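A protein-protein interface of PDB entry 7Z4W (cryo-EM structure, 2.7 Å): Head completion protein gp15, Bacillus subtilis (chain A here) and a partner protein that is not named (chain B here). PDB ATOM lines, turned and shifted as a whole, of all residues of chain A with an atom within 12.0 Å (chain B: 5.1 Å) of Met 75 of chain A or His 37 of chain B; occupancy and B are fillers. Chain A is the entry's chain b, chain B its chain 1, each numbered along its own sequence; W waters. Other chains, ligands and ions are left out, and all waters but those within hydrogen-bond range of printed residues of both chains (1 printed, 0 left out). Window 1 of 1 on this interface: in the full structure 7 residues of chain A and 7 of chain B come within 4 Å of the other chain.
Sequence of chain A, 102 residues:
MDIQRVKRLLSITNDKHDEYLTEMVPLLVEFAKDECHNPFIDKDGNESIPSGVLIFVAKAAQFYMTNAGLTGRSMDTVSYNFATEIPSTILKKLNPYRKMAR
OG of Ser 74 of chain A lies within hydrogen-bond range of O of Val 78 of chain A (3.4 Å).
The backbone carbonyl oxygen (O) of Arg 73 of chain A sits at hydrogen-bond distance from the backbone NH (N) of Tyr 80 of chain A (2.9 Å).
The backbone NH (N) of His 37 of chain B is in hydrogen-bond range of the backbone carbonyl oxygen (O) of Tyr 61 of chain B (2.9 Å).
ND1 of His 37 of chain B lies within hydrogen-bond range of NE2 of Gln 39 of chain B, at 3.1 Å.
The backbone carbonyl oxygen of Gln 39 of chain B is in hydrogen-bond range of the backbone NH of Asn 59 of chain B.
O of Met 75 of chain A lies within hydrogen-bond range of NE2 of Gln 39 of chain B, at 3.4 Å.
OD2 of Asp 76 of chain A lies close to OE1 of Gln 39 of chain B (3.3 Å).
OG1 of Thr 77 of chain A sits close to OE1 of Gln 39 of chain B, 2.3 Å away.
OD1 of Asp 76 of chain A lies close to OH of Tyr 61 of chain B (3.4 Å).
Of the printed residues of chain B, Arg 73 of chain A touches Glu 4 (3.4 Å).
Of the printed residues of chain B, Met 75 of chain A touches Glu 4, His 37 and Gln 39.
Of the printed residues of chain B, Asp 76 of chain A touches Gln 39 (3.3 Å) and Tyr 61 (3.2 Å).
Of the printed residues of chain B, Thr 77 of chain A touches Gln 39 (2.3 Å).
Of the printed residues of chain B, Val 78 of chain A touches His 37 (3.996 Å).
Ser 79 of chain A touches none of the printed residues of chain B.
Asn 81 of chain A touches none of the printed residues of chain B.
Of the printed residues of chain A, Glu 4 of chain B touches Arg 73 and Met 75.
Pro 6 of chain B touches none of the printed residues of chain A.
No residue of chain A comes within 4 Å of Asp 7 of chain B.
Printed residues of chain A within 4 Å of His 37 of chain B: Met 75 (3.4 Å) and Val 78 (3.996 Å).
No residue of chain A comes within 4 Å of Val 38 of chain B.
Gln 39 of chain B touches three residues of chain A.
Of the printed residues of chain A, Tyr 61 of chain B touches Asp 76.
The nearest printed residue of chain B that does not touch Met 75 of chain A is Tyr 61 of chain B (4.02 Å).
The nearest printed residue of chain B that does not touch Arg 73 of chain A is Phe 5 of chain B (6.1 Å).
Of the 13 printed residues of chain A, 5 touch a printed residue of chain B.
Hydrophobic or aromatic side chains of chain A within 4 Å of the printed part of chain B: Met 75 and Val 78.
Along chain A the printed residues that touch a printed residue of chain B span positions 73 to 78.
Among the printed residues, 8 pairs touch across the chains.
Among the printed residues, no Asp or Glu carboxylate lies within 4 Å of a Lys or Arg side-chain nitrogen of the other chain.
Water W1 lies within hydrogen-bond range of ND1 of His 37 of chain B (3.1 Å), O of Glu 4 of chain B (3.3 Å) and NH2 of Arg 73 of chain A (3.4 Å).
Among the printed residues, pairs that only touch across the chains: Met 75 of chain A with Glu 4 of chain B (3.3 Å), Met 75 of chain A with His 37 of chain B (3.4 Å), Arg 73 of chain A with Glu 4 of chain B (3.4 Å) and Val 78 of chain A with His 37 of chain B (3.996 Å).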
ATOM      1  N   LEU A  70      12.465  -2.883  -3.901  1.00  0.00           N
ATOM      2  CA  LEU A  70      12.940  -3.277  -2.580  1.00  0.00           C
ATOM      3  C   LEU A  70      13.962  -2.271  -2.073  1.00  0.00           C
ATOM      4  O   LEU A  70      14.906  -1.935  -2.790  1.00  0.00           O
ATOM      5  CB  LEU A  70      13.559  -4.679  -2.631  1.00  0.00           C
ATOM      6  CG  LEU A  70      13.440  -5.581  -1.408  1.00  0.00           C
ATOM      7  CD1 LEU A  70      11.991  -5.940  -1.149  1.00  0.00           C
ATOM      8  CD2 LEU A  70      14.272  -6.837  -1.606  1.00  0.00           C
ATOM      9  N   THR A  71      13.773  -1.792  -0.841  1.00  0.00           N
ATOM     10  CA  THR A  71      14.756  -0.930  -0.196  1.00  0.00           C
ATOM     11  C   THR A  71      15.532  -1.609   0.924  1.00  0.00           C
ATOM     12  O   THR A  71      16.580  -1.093   1.320  1.00  0.00           O
ATOM     13  CB  THR A  71      14.090   0.340   0.362  1.00  0.00           C
ATOM     14  OG1 THR A  71      13.180   0.000   1.412  1.00  0.00           O
ATOM     15  CG2 THR A  71      13.339   1.078  -0.729  1.00  0.00           C
ATOM     16  N   GLY A  72      15.053  -2.738   1.443  1.00  0.00           N
ATOM     17  CA  GLY A  72      15.755  -3.439   2.501  1.00  0.00           C
ATOM     18  C   GLY A  72      15.294  -4.873   2.607  1.00  0.00           C
ATOM     19  O   GLY A  72      14.169  -5.214   2.235  1.00  0.00           O
ATOM     20  N   ARG A  73      16.181  -5.716   3.134  1.00  0.00           N
ATOM     21  CA  ARG A  73      15.920  -7.148   3.222  1.00  0.00           C
ATOM     22  C   ARG A  73      16.700  -7.725   4.396  1.00  0.00           C
ATOM     23  O   ARG A  73      17.753  -7.205   4.760  1.00  0.00           O
ATOM     24  CB  ARG A  73      16.303  -7.847   1.909  1.00  0.00           C
ATOM     25  CG  ARG A  73      15.736  -9.229   1.733  1.00  0.00           C
ATOM     26  CD  ARG A  73      15.931  -9.769   0.319  1.00  0.00           C
ATOM     27  NE  ARG A  73      17.328  -9.924  -0.084  1.00  0.00           N
ATOM     28  CZ  ARG A  73      18.149 -10.889   0.327  1.00  0.00           C
ATOM     29  NH1 ARG A  73      19.390 -10.930  -0.127  1.00  0.00           N
ATOM     30  NH2 ARG A  73      17.748 -11.809   1.192  1.00  0.00           N
ATOM     31  N   SER A  74      16.178  -8.796   4.998  1.00  0.00           N
ATOM     32  CA  SER A  74      16.848  -9.420   6.136  1.00  0.00           C
ATOM     33  C   SER A  74      16.476 -10.893   6.242  1.00  0.00           C
ATOM     34  O   SER A  74      15.298 -11.238   6.147  1.00  0.00           O
ATOM     35  CB  SER A  74      16.488  -8.699   7.436  1.00  0.00           C
ATOM     36  OG  SER A  74      17.123  -9.305   8.541  1.00  0.00           O
ATOM     37  N   MET A  75      17.481 -11.758   6.424  1.00  0.00           N
ATOM     38  CA  MET A  75      17.261 -13.183   6.708  1.00  0.00           C
ATOM     39  C   MET A  75      18.245 -13.650   7.785  1.00  0.00           C
ATOM     40  O   MET A  75      19.393 -14.002   7.493  1.00  0.00           O
ATOM     41  CB  MET A  75      17.371 -14.019   5.443  1.00  0.00           C
ATOM     42  CG  MET A  75      16.913 -15.452   5.631  1.00  0.00           C
ATOM     43  SD  MET A  75      16.180 -16.152   4.148  1.00  0.00           S
ATOM     44  CE  MET A  75      17.648 -16.533   3.225  1.00  0.00           C
ATOM     45  N   ASP A  76      17.823 -13.521   9.044  1.00  0.00           N
ATOM     46  CA  ASP A  76      18.257 -14.271  10.226  1.00  0.00           C
ATOM     47  C   ASP A  76      19.688 -14.041  10.716  1.00  0.00           C
ATOM     48  O   ASP A  76      19.935 -14.092  11.924  1.00  0.00           O
ATOM     49  CB  ASP A  76      18.067 -15.768   9.943  1.00  0.00           C
ATOM     50  CG  ASP A  76      18.530 -16.649  11.086  1.00  0.00           C
ATOM     51  OD1 ASP A  76      17.908 -16.612  12.166  1.00  0.00           O
ATOM     52  OD2 ASP A  76      19.526 -17.377  10.905  1.00  0.00           O
ATOM     53  N   THR A  77      20.601 -13.654   9.832  1.00  0.00           N
ATOM     54  CA  THR A  77      21.957 -13.255  10.194  1.00  0.00           C
ATOM     55  C   THR A  77      22.383 -12.201   9.192  1.00  0.00           C
ATOM     56  O   THR A  77      23.252 -11.374   9.474  1.00  0.00           O
ATOM     57  CB  THR A  77      22.966 -14.421  10.191  1.00  0.00           C
ATOM     58  OG1 THR A  77      22.747 -15.279   9.066  1.00  0.00           O
ATOM     59  CG2 THR A  77      22.945 -15.226  11.488  1.00  0.00           C
ATOM     60  N   VAL A  78      21.770 -12.237   8.016  1.00  0.00           N
ATOM     61  CA  VAL A  78      22.146 -11.363   6.916  1.00  0.00           C
ATOM     62  C   VAL A  78      21.122 -10.240   6.816  1.00  0.00           C
ATOM     63  O   VAL A  78      19.939 -10.436   7.096  1.00  0.00           O
ATOM     64  CB  VAL A  78      22.245 -12.176   5.607  1.00  0.00           C
ATOM     65  CG1 VAL A  78      23.008 -11.419   4.565  1.00  0.00           C
ATOM     66  CG2 VAL A  78      22.899 -13.516   5.865  1.00  0.00           C
ATOM     67  N   SER A  79      21.575  -9.047   6.429  1.00  0.00           N
ATOM     68  CA  SER A  79      20.666  -7.944   6.152  1.00  0.00           C
ATOM     69  C   SER A  79      21.301  -7.009   5.131  1.00  0.00           C
ATOM     70  O   SER A  79      22.525  -6.904   5.042  1.00  0.00           O
ATOM     71  CB  SER A  79      20.293  -7.177   7.426  1.00  0.00           C
ATOM     72  OG  SER A  79      21.202  -6.129   7.688  1.00  0.00           O
ATOM     73  N   TYR A  80      20.448  -6.330   4.364  1.00  0.00           N
ATOM     74  CA  TYR A  80      20.865  -5.432   3.297  1.00  0.00           C
ATOM     75  C   TYR A  80      19.986  -4.194   3.271  1.00  0.00           C
ATOM     76  O   TYR A  80      18.765  -4.283   3.438  1.00  0.00           O
ATOM     77  CB  TYR A  80      20.789  -6.093   1.919  1.00  0.00           C
ATOM     78  CG  TYR A  80      21.633  -7.320   1.769  1.00  0.00           C
ATOM     79  CD1 TYR A  80      23.001  -7.221   1.568  1.00  0.00           C
ATOM     80  CD2 TYR A  80      21.064  -8.580   1.828  1.00  0.00           C
ATOM     81  CE1 TYR A  80      23.778  -8.345   1.433  1.00  0.00           C
ATOM     82  CE2 TYR A  80      21.828  -9.705   1.691  1.00  0.00           C
ATOM     83  CZ  TYR A  80      23.186  -9.585   1.496  1.00  0.00           C
ATOM     84  OH  TYR A  80      23.950 -10.718   1.361  1.00  0.00           O
ATOM     85  N   ASN A  81      20.623  -3.050   3.030  1.00  0.00           N
ATOM     86  CA  ASN A  81      19.955  -1.792   2.731  1.00  0.00           C
ATOM     87  C   ASN A  81      20.404  -1.334   1.353  1.00  0.00           C
ATOM     88  O   ASN A  81      21.605  -1.218   1.098  1.00  0.00           O
ATOM     89  CB  ASN A  81      20.282  -0.722   3.773  1.00  0.00           C
ATOM     90  CG  ASN A  81      19.669  -1.017   5.119  1.00  0.00           C
ATOM     91  OD1 ASN A  81      18.458  -0.917   5.297  1.00  0.00           O
ATOM     92  ND2 ASN A  81      20.504  -1.384   6.078  1.00  0.00           N
ATOM     93  N   PHE A  82      19.447  -1.077   0.471  1.00  0.00           N
ATOM     94  CA  PHE A  82      19.737  -0.772  -0.921  1.00  0.00           C
ATOM     95  C   PHE A  82      19.573   0.716  -1.205  1.00  0.00           C
ATOM     96  O   PHE A  82      18.787   1.410  -0.557  1.00  0.00           O
ATOM     97  CB  PHE A  82      18.831  -1.579  -1.854  1.00  0.00           C
ATOM     98  CG  PHE A  82      18.919  -3.063  -1.650  1.00  0.00           C
ATOM     99  CD1 PHE A  82      20.062  -3.758  -2.012  1.00  0.00           C
ATOM    100  CD2 PHE A  82      17.859  -3.766  -1.101  1.00  0.00           C
ATOM    101  CE1 PHE A  82      20.145  -5.126  -1.828  1.00  0.00           C
ATOM    102  CE2 PHE A  82      17.937  -5.132  -0.913  1.00  0.00           C
ATOM    103  CZ  PHE A  82      19.081  -5.811  -1.279  1.00  0.00           C
ATOM    104  N   GLU B   4      18.301 -14.237  -2.423  1.00  0.00           N
ATOM    105  CA  GLU B   4      17.895 -14.798  -1.141  1.00  0.00           C
ATOM    106  C   GLU B   4      18.375 -16.233  -0.995  1.00  0.00           C
ATOM    107  O   GLU B   4      18.754 -16.657   0.099  1.00  0.00           O
ATOM    108  CB  GLU B   4      16.378 -14.739  -0.988  1.00  0.00           C
ATOM    109  CG  GLU B   4      15.777 -13.367  -1.130  1.00  0.00           C
ATOM    110  CD  GLU B   4      14.328 -13.333  -0.691  1.00  0.00           C
ATOM    111  OE1 GLU B   4      14.054 -13.655   0.484  1.00  0.00           O
ATOM    112  OE2 GLU B   4      13.461 -12.991  -1.521  1.00  0.00           O
ATOM    113  N   PHE B   5      18.373 -16.965  -2.084  1.00  0.00           N
ATOM    114  CA  PHE B   5      18.773 -18.343  -2.090  1.00  0.00           C
ATOM    115  C   PHE B   5      19.922 -18.565  -3.040  1.00  0.00           C
ATOM    116  O   PHE B   5      19.704 -18.864  -4.160  1.00  0.00           O
ATOM    117  CB  PHE B   5      17.567 -19.175  -2.480  1.00  0.00           C
ATOM    118  CG  PHE B   5      16.378 -18.940  -1.616  1.00  0.00           C
ATOM    119  CD1 PHE B   5      16.361 -19.358  -0.307  1.00  0.00           C
ATOM    120  CD2 PHE B   5      15.285 -18.289  -2.101  1.00  0.00           C
ATOM    121  CE1 PHE B   5      15.284 -19.138   0.492  1.00  0.00           C
ATOM    122  CE2 PHE B   5      14.197 -18.061  -1.309  1.00  0.00           C
ATOM    123  CZ  PHE B   5      14.193 -18.490  -0.011  1.00  0.00           C
ATOM    124  N   PRO B   6      21.158 -18.435  -2.584  1.00  0.00           N
ATOM    125  CA  PRO B   6      22.305 -18.585  -3.483  1.00  0.00           C
ATOM    126  C   PRO B   6      22.865 -19.994  -3.606  1.00  0.00           C
ATOM    127  O   PRO B   6      23.723 -20.210  -4.468  1.00  0.00           O
ATOM    128  CB  PRO B   6      23.339 -17.646  -2.847  1.00  0.00           C
ATOM    129  CG  PRO B   6      23.044 -17.720  -1.410  1.00  0.00           C
ATOM    130  CD  PRO B   6      21.555 -17.854  -1.289  1.00  0.00           C
ATOM    131  N   ASP B   7      22.420 -20.948  -2.796  1.00  0.00           N
ATOM    132  CA  ASP B   7      22.946 -22.304  -2.825  1.00  0.00           C
ATOM    133  C   ASP B   7      22.007 -23.244  -3.573  1.00  0.00           C
ATOM    134  O   ASP B   7      20.883 -22.896  -3.930  1.00  0.00           O
ATOM    135  CB  ASP B   7      23.182 -22.826  -1.407  1.00  0.00           C
ATOM    136  CG  ASP B   7      24.131 -21.959  -0.614  1.00  0.00           C
ATOM    137  OD1 ASP B   7      25.012 -21.323  -1.221  1.00  0.00           O
ATOM    138  OD2 ASP B   7      24.002 -21.918   0.625  1.00  0.00           O
ATOM    139  N   ALA B  35      16.730 -24.463  -4.672  1.00  0.00           N
ATOM    140  CA  ALA B  35      17.539 -23.330  -4.248  1.00  0.00           C
ATOM    141  C   ALA B  35      17.336 -23.077  -2.761  1.00  0.00           C
ATOM    142  O   ALA B  35      16.230 -23.221  -2.241  1.00  0.00           O
ATOM    143  CB  ALA B  35      17.173 -22.083  -5.046  1.00  0.00           C
ATOM    144  N   ALA B  36      18.410 -22.704  -2.075  1.00  0.00           N
ATOM    145  CA  ALA B  36      18.361 -22.599  -0.625  1.00  0.00           C
ATOM    146  C   ALA B  36      19.424 -21.630  -0.141  1.00  0.00           C
ATOM    147  O   ALA B  36      20.259 -21.152  -0.908  1.00  0.00           O
ATOM    148  CB  ALA B  36      18.550 -23.966   0.038  1.00  0.00           C
ATOM    149  N   HIS B  37      19.372 -21.346   1.155  1.00  0.00           N
ATOM    150  CA  HIS B  37      20.430 -20.634   1.860  1.00  0.00           C
ATOM    151  C   HIS B  37      20.742 -21.402   3.134  1.00  0.00           C
ATOM    152  O   HIS B  37      19.873 -21.552   3.999  1.00  0.00           O
ATOM    153  CB  HIS B  37      20.028 -19.191   2.176  1.00  0.00           C
ATOM    154  CG  HIS B  37      21.175 -18.320   2.586  1.00  0.00           C
ATOM    155  ND1 HIS B  37      21.009 -17.022   3.015  1.00  0.00           N
ATOM    156  CD2 HIS B  37      22.506 -18.563   2.635  1.00  0.00           C
ATOM    157  CE1 HIS B  37      22.187 -16.501   3.306  1.00  0.00           C
ATOM    158  NE2 HIS B  37      23.111 -17.415   3.085  1.00  0.00           N
ATOM    159  N   VAL B  38      21.969 -21.900   3.234  1.00  0.00           N
ATOM    160  CA  VAL B  38      22.423 -22.687   4.374  1.00  0.00           C
ATOM    161  C   VAL B  38      23.274 -21.782   5.252  1.00  0.00           C
ATOM    162  O   VAL B  38      24.330 -21.304   4.821  1.00  0.00           O
ATOM    163  CB  VAL B  38      23.213 -23.924   3.918  1.00  0.00           C
ATOM    164  CG1 VAL B  38      23.577 -24.798   5.106  1.00  0.00           C
ATOM    165  CG2 VAL B  38      22.429 -24.709   2.887  1.00  0.00           C
ATOM    166  N   GLN B  39      22.823 -21.538   6.482  1.00  0.00           N
ATOM    167  CA  GLN B  39      23.498 -20.624   7.380  1.00  0.00           C
ATOM    168  C   GLN B  39      23.916 -21.336   8.659  1.00  0.00           C
ATOM    169  O   GLN B  39      23.120 -22.077   9.242  1.00  0.00           O
ATOM    170  CB  GLN B  39      22.589 -19.440   7.744  1.00  0.00           C
ATOM    171  CG  GLN B  39      22.265 -18.503   6.599  1.00  0.00           C
ATOM    172  CD  GLN B  39      21.385 -17.352   7.036  1.00  0.00           C
ATOM    173  OE1 GLN B  39      21.421 -16.935   8.187  1.00  0.00           O
ATOM    174  NE2 GLN B  39      20.583 -16.837   6.117  1.00  0.00           N
ATOM    175  N   ASN B  59      20.914 -23.760  10.045  1.00  0.00           N
ATOM    176  CA  ASN B  59      19.562 -23.409   9.628  1.00  0.00           C
ATOM    177  C   ASN B  59      19.526 -23.341   8.105  1.00  0.00           C
ATOM    178  O   ASN B  59      20.368 -22.682   7.489  1.00  0.00           O
ATOM    179  CB  ASN B  59      19.126 -22.063  10.217  1.00  0.00           C
ATOM    180  CG  ASN B  59      18.776 -22.150  11.687  1.00  0.00           C
ATOM    181  OD1 ASN B  59      18.126 -23.093  12.130  1.00  0.00           O
ATOM    182  ND2 ASN B  59      19.205 -21.159  12.451  1.00  0.00           N
ATOM    183  N   ILE B  60      18.552 -24.011   7.501  1.00  0.00           N
ATOM    184  CA  ILE B  60      18.411 -24.074   6.052  1.00  0.00           C
ATOM    185  C   ILE B  60      17.102 -23.398   5.686  1.00  0.00           C
ATOM    186  O   ILE B  60      16.037 -23.804   6.164  1.00  0.00           O
ATOM    187  CB  ILE B  60      18.442 -25.522   5.538  1.00  0.00           C
ATOM    188  CG1 ILE B  60      19.705 -26.236   6.019  1.00  0.00           C
ATOM    189  CG2 ILE B  60      18.355 -25.551   4.033  1.00  0.00           C
ATOM    190  CD1 ILE B  60      19.737 -27.704   5.689  1.00  0.00           C
ATOM    191  N   TYR B  61      17.175 -22.372   4.844  1.00  0.00           N
ATOM    192  CA  TYR B  61      15.995 -21.660   4.373  1.00  0.00           C
ATOM    193  C   TYR B  61      15.765 -21.999   2.910  1.00  0.00           C
ATOM    194  O   TYR B  61      16.695 -21.942   2.103  1.00  0.00           O
ATOM    195  CB  TYR B  61      16.150 -20.148   4.561  1.00  0.00           C
ATOM    196  CG  TYR B  61      16.166 -19.732   6.013  1.00  0.00           C
ATOM    197  CD1 TYR B  61      14.986 -19.444   6.684  1.00  0.00           C
ATOM    198  CD2 TYR B  61      17.362 -19.643   6.715  1.00  0.00           C
ATOM    199  CE1 TYR B  61      14.995 -19.073   8.012  1.00  0.00           C
ATOM    200  CE2 TYR B  61      17.380 -19.275   8.043  1.00  0.00           C
ATOM    201  CZ  TYR B  61      16.195 -18.990   8.686  1.00  0.00           C
ATOM    202  OH  TYR B  61      16.212 -18.620  10.008  1.00  0.00           O
HETATM  203  O   HOH W   1      19.890 -14.288   2.147  1.00  0.00           O
